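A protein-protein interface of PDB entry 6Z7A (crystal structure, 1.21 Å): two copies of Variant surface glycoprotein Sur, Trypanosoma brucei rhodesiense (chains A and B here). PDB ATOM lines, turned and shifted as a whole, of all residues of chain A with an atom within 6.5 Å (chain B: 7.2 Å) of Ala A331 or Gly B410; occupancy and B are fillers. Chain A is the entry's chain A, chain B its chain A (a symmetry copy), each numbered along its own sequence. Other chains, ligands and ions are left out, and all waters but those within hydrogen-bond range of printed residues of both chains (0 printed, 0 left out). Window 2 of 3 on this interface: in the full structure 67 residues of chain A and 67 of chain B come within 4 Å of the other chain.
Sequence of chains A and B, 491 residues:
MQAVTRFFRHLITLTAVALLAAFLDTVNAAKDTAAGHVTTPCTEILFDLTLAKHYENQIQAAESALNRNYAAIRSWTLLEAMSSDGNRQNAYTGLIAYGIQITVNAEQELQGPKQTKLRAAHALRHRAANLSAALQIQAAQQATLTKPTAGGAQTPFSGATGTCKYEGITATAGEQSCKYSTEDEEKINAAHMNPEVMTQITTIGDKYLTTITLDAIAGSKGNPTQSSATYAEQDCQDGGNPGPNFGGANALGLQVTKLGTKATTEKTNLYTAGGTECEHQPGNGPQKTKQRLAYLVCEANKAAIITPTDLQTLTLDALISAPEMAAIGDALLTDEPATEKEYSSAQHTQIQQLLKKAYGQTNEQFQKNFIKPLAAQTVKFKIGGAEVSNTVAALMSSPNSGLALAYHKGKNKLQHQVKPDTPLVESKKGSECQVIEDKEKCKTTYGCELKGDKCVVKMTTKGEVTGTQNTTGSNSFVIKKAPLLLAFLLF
Among the printed residues, merely in contact across the chains: Ala A331 with Gly B410 (3.4 Å), Ala A327 with Leu B403 (3.5 Å), Ala A331 with Ala B406 (3.7 Å), Leu A332 with Ala B406 (3.8 Å), Ala A331 with Tyr B407 (3.8 Å), Thr A93 with Lys B409 (3.9 Å), Ile A328 with Leu B403 (3.9 Å) and Leu A332 with Gly B410 (3.9 Å).
Printed residues of chain B within 4 Å of Ile A328: Leu B403. Ala A331 touches three residues of chain B. Of the printed residues of chain A, Ala B406 touches Ala A331 and Leu A332. Of the printed residues of chain A, Tyr B407 touches Ala A331. Of chain A, only Ala A331 (3.4 Å) and Leu A332 (3.9 Å) come within 4 Å of Gly B410. The nearest residue of chain A that does not touch Gly B410 is Asn A90 (6.0 Å). The nearest printed residue of chain A that does not touch Lys B409 is Leu A332 (4.1 Å).
Hydrophobic or aromatic side chains of chain A that line the printed part of chain B: Ala A327, Ala A331 and Leu A332. Printed residues of chain B that touch a printed residue of chain A: Leu B403, Ala B406, Tyr B407, Lys B409 and Gly B410. Among the printed residues, no Asp or Glu carboxylate lies within 4 Å of a Lys or Arg side-chain nitrogen of the other chain.
No position is printed for both chains. Of the 8 pairs that touch across the chains among the printed residues, none has its exchanged pair printed and touching as well.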
ATOM      1  N   ASN A  90      20.789  -8.755  -9.112  1.00  0.00           N
ATOM      2  CA  ASN A  90      21.578  -8.957 -10.323  1.00  0.00           C
ATOM      3  C   ASN A  90      23.065  -8.907 -10.007  1.00  0.00           C
ATOM      4  O   ASN A  90      23.847  -9.632 -10.614  1.00  0.00           O
ATOM      5  CB  ASN A  90      21.235  -7.929 -11.427  1.00  0.00           C
ATOM      6  CG  ASN A  90      19.887  -8.199 -12.090  1.00  0.00           C
ATOM      7  OD1 ASN A  90      19.347  -9.300 -12.008  1.00  0.00           O
ATOM      8  ND2 ASN A  90      19.335  -7.171 -12.755  1.00  0.00           N
ATOM      9  N   THR A  93      24.036 -12.161  -8.576  1.00  0.00           N
ATOM     10  CA  THR A  93      24.035 -13.117  -9.665  1.00  0.00           C
ATOM     11  C   THR A  93      25.300 -12.993 -10.482  1.00  0.00           C
ATOM     12  O   THR A  93      25.876 -14.001 -10.895  1.00  0.00           O
ATOM     13  CB  THR A  93      22.772 -12.902 -10.538  1.00  0.00           C
ATOM     14  OG1 THR A  93      21.619 -13.146  -9.741  1.00  0.00           O
ATOM     15  CG2 THR A  93      22.790 -13.914 -11.673  1.00  0.00           C
ATOM     16  N   ALA A 326      33.519  -8.972 -18.298  1.00  0.00           N
ATOM     17  CA  ALA A 326      33.026  -8.200 -19.437  1.00  0.00           C
ATOM     18  C   ALA A 326      31.725  -8.794 -19.971  1.00  0.00           C
ATOM     19  O   ALA A 326      30.696  -8.107 -20.030  1.00  0.00           O
ATOM     20  CB  ALA A 326      34.111  -8.144 -20.523  1.00  0.00           C
ATOM     21  N   ALA A 327      31.730 -10.090 -20.312  1.00  0.00           N
ATOM     22  CA  ALA A 327      30.518 -10.706 -20.869  1.00  0.00           C
ATOM     23  C   ALA A 327      29.431 -10.859 -19.806  1.00  0.00           C
ATOM     24  O   ALA A 327      28.254 -10.698 -20.087  1.00  0.00           O
ATOM     25  CB  ALA A 327      30.852 -12.073 -21.481  1.00  0.00           C
ATOM     26  N   ILE A 328      29.813 -11.225 -18.581  1.00  0.00           N
ATOM     27  CA  ILE A 328      28.840 -11.374 -17.509  1.00  0.00           C
ATOM     28  C   ILE A 328      28.170 -10.040 -17.213  1.00  0.00           C
ATOM     29  O   ILE A 328      26.944  -9.966 -17.075  1.00  0.00           O
ATOM     30  CB  ILE A 328      29.524 -11.986 -16.270  1.00  0.00           C
ATOM     31  CG1 ILE A 328      29.746 -13.503 -16.495  1.00  0.00           C
ATOM     32  CG2 ILE A 328      28.717 -11.693 -15.008  1.00  0.00           C
ATOM     33  CD1 ILE A 328      30.736 -14.142 -15.504  1.00  0.00           C
ATOM     34  N   GLY A 329      28.966  -8.977 -17.111  1.00  0.00           N
ATOM     35  CA  GLY A 329      28.398  -7.646 -16.943  1.00  0.00           C
ATOM     36  C   GLY A 329      27.495  -7.233 -18.095  1.00  0.00           C
ATOM     37  O   GLY A 329      26.410  -6.677 -17.882  1.00  0.00           O
ATOM     38  N   ASP A 330      27.931  -7.488 -19.332  1.00  0.00           N
ATOM     39  CA  ASP A 330      27.088  -7.167 -20.481  1.00  0.00           C
ATOM     40  C   ASP A 330      25.765  -7.912 -20.390  1.00  0.00           C
ATOM     41  O   ASP A 330      24.717  -7.381 -20.761  1.00  0.00           O
ATOM     42  CB  ASP A 330      27.813  -7.549 -21.774  1.00  0.00           C
ATOM     43  CG  ASP A 330      27.003  -7.177 -23.021  1.00  0.00           C
ATOM     44  OD1 ASP A 330      26.342  -6.111 -23.003  1.00  0.00           O
ATOM     45  OD2 ASP A 330      27.014  -7.951 -24.004  1.00  0.00           O
ATOM     46  N   ALA A 331      25.788  -9.144 -19.872  1.00  0.00           N
ATOM     47  CA  ALA A 331      24.579  -9.963 -19.833  1.00  0.00           C
ATOM     48  C   ALA A 331      23.593  -9.514 -18.760  1.00  0.00           C
ATOM     49  O   ALA A 331      22.371  -9.617 -18.964  1.00  0.00           O
ATOM     50  CB  ALA A 331      24.948 -11.435 -19.573  1.00  0.00           C
ATOM     51  N   LEU A 332      24.088  -8.993 -17.640  1.00  0.00           N
ATOM     52  CA  LEU A 332      23.270  -8.685 -16.481  1.00  0.00           C
ATOM     53  C   LEU A 332      23.024  -7.190 -16.314  1.00  0.00           C
ATOM     54  O   LEU A 332      22.030  -6.820 -15.681  1.00  0.00           O
ATOM     55  CB  LEU A 332      23.914  -9.234 -15.196  1.00  0.00           C
ATOM     56  CG  LEU A 332      23.736 -10.721 -14.966  1.00  0.00           C
ATOM     57  CD1 LEU A 332      24.814 -11.253 -13.928  1.00  0.00           C
ATOM     58  CD2 LEU A 332      22.321 -11.054 -14.493  1.00  0.00           C
ATOM     59  N   LEU A 333      23.911  -6.353 -16.860  1.00  0.00           N
ATOM     60  CA  LEU A 333      23.876  -4.912 -16.716  1.00  0.00           C
ATOM     61  C   LEU A 333      23.648  -4.266 -18.089  1.00  0.00           C
ATOM     62  O   LEU A 333      23.135  -3.166 -18.193  1.00  0.00           O
ATOM     63  CB  LEU A 333      25.213  -4.458 -16.109  1.00  0.00           C
ATOM     64  CG  LEU A 333      25.780  -5.324 -14.982  1.00  0.00           C
ATOM     65  CD1 LEU A 333      27.142  -4.808 -14.492  1.00  0.00           C
ATOM     66  CD2 LEU A 333      24.814  -5.375 -13.839  1.00  0.00           C
ATOM     67  N   ALA B  81      16.795 -20.322 -13.801  1.00  0.00           N
ATOM     68  CA  ALA B  81      16.973 -19.045 -14.500  1.00  0.00           C
ATOM     69  C   ALA B  81      16.234 -18.991 -15.831  1.00  0.00           C
ATOM     70  O   ALA B  81      15.875 -17.892 -16.292  1.00  0.00           O
ATOM     71  CB  ALA B  81      18.479 -18.881 -14.754  1.00  0.00           C
ATOM     72  N   LEU B 403      28.682 -17.999 -17.530  1.00  0.00           N
ATOM     73  CA  LEU B 403      28.157 -17.041 -18.492  1.00  0.00           C
ATOM     74  C   LEU B 403      26.765 -17.438 -18.965  1.00  0.00           C
ATOM     75  O   LEU B 403      25.883 -16.580 -19.125  1.00  0.00           O
ATOM     76  CB  LEU B 403      29.129 -16.953 -19.653  1.00  0.00           C
ATOM     77  CG  LEU B 403      28.792 -15.970 -20.764  1.00  0.00           C
ATOM     78  CD1 LEU B 403      28.674 -14.531 -20.241  1.00  0.00           C
ATOM     79  CD2 LEU B 403      29.869 -16.101 -21.795  1.00  0.00           C
ATOM     80  N   ALA B 404      26.544 -18.740 -19.172  1.00  0.00           N
ATOM     81  CA  ALA B 404      25.198 -19.230 -19.500  1.00  0.00           C
ATOM     82  C   ALA B 404      24.190 -18.805 -18.441  1.00  0.00           C
ATOM     83  O   ALA B 404      23.081 -18.376 -18.763  1.00  0.00           O
ATOM     84  CB  ALA B 404      25.212 -20.759 -19.618  1.00  0.00           C
ATOM     85  N   LEU B 405      24.563 -18.918 -17.168  1.00  0.00           N
ATOM     86  CA  LEU B 405      23.691 -18.460 -16.096  1.00  0.00           C
ATOM     87  C   LEU B 405      23.450 -16.958 -16.183  1.00  0.00           C
ATOM     88  O   LEU B 405      22.305 -16.498 -16.103  1.00  0.00           O
ATOM     89  CB  LEU B 405      24.319 -18.811 -14.754  1.00  0.00           C
ATOM     90  CG  LEU B 405      23.543 -18.427 -13.526  1.00  0.00           C
ATOM     91  CD1 LEU B 405      22.142 -19.060 -13.575  1.00  0.00           C
ATOM     92  CD2 LEU B 405      24.363 -18.826 -12.241  1.00  0.00           C
ATOM     93  N   ALA B 406      24.513 -16.167 -16.299  1.00  0.00           N
ATOM     94  CA  ALA B 406      24.336 -14.702 -16.385  1.00  0.00           C
ATOM     95  C   ALA B 406      23.469 -14.326 -17.564  1.00  0.00           C
ATOM     96  O   ALA B 406      22.609 -13.448 -17.445  1.00  0.00           O
ATOM     97  CB  ALA B 406      25.709 -13.999 -16.492  1.00  0.00           C
ATOM     98  N   TYR B 407      23.659 -15.001 -18.701  1.00  0.00           N
ATOM     99  CA  TYR B 407      22.912 -14.641 -19.898  1.00  0.00           C
ATOM    100  C   TYR B 407      21.426 -14.852 -19.688  1.00  0.00           C
ATOM    101  O   TYR B 407      20.611 -13.978 -20.004  1.00  0.00           O
ATOM    102  CB  TYR B 407      23.412 -15.464 -21.083  1.00  0.00           C
ATOM    103  CG  TYR B 407      22.578 -15.223 -22.313  1.00  0.00           C
ATOM    104  CD1 TYR B 407      22.660 -14.020 -22.994  1.00  0.00           C
ATOM    105  CD2 TYR B 407      21.689 -16.180 -22.767  1.00  0.00           C
ATOM    106  CE1 TYR B 407      21.900 -13.783 -24.063  1.00  0.00           C
ATOM    107  CE2 TYR B 407      20.886 -15.933 -23.892  1.00  0.00           C
ATOM    108  CZ  TYR B 407      21.012 -14.735 -24.531  1.00  0.00           C
ATOM    109  OH  TYR B 407      20.237 -14.445 -25.648  1.00  0.00           O
ATOM    110  N   HIS B 408      21.051 -16.001 -19.136  1.00  0.00           N
ATOM    111  CA  HIS B 408      19.634 -16.292 -18.992  1.00  0.00           C
ATOM    112  C   HIS B 408      19.016 -15.553 -17.818  1.00  0.00           C
ATOM    113  O   HIS B 408      17.846 -15.199 -17.876  1.00  0.00           O
ATOM    114  CB  HIS B 408      19.401 -17.804 -18.882  1.00  0.00           C
ATOM    115  CG  HIS B 408      19.676 -18.528 -20.157  1.00  0.00           C
ATOM    116  ND1 HIS B 408      20.913 -19.054 -20.469  1.00  0.00           N
ATOM    117  CD2 HIS B 408      18.896 -18.715 -21.253  1.00  0.00           C
ATOM    118  CE1 HIS B 408      20.858 -19.598 -21.677  1.00  0.00           C
ATOM    119  NE2 HIS B 408      19.648 -19.408 -22.169  1.00  0.00           N
ATOM    120  N   LYS B 409      19.768 -15.300 -16.754  1.00  0.00           N
ATOM    121  CA  LYS B 409      19.245 -14.478 -15.669  1.00  0.00           C
ATOM    122  C   LYS B 409      19.012 -13.046 -16.132  1.00  0.00           C
ATOM    123  O   LYS B 409      18.078 -12.397 -15.657  1.00  0.00           O
ATOM    124  CB  LYS B 409      20.187 -14.539 -14.442  1.00  0.00           C
ATOM    125  CG  LYS B 409      19.889 -15.730 -13.500  1.00  0.00           C
ATOM    126  CD  LYS B 409      18.810 -15.465 -12.383  1.00  0.00           C
ATOM    127  CE  LYS B 409      19.189 -16.262 -11.088  1.00  0.00           C
ATOM    128  NZ  LYS B 409      18.076 -16.456 -10.083  1.00  0.00           N
ATOM    129  N   GLY B 410      19.825 -12.563 -17.079  1.00  0.00           N
ATOM    130  CA  GLY B 410      19.624 -11.234 -17.650  1.00  0.00           C
ATOM    131  C   GLY B 410      18.485 -11.153 -18.644  1.00  0.00           C
ATOM    132  O   GLY B 410      17.866 -10.093 -18.777  1.00  0.00           O
ATOM    133  N   LYS B 411      18.237 -12.234 -19.387  1.00  0.00           N
ATOM    134  CA  LYS B 411      17.150 -12.319 -20.357  1.00  0.00           C
ATOM    135  C   LYS B 411      15.946 -12.925 -19.654  1.00  0.00           C
ATOM    136  O   LYS B 411      15.214 -12.218 -18.953  1.00  0.00           O
ATOM    137  CB  LYS B 411      17.563 -13.185 -21.560  1.00  0.00           C
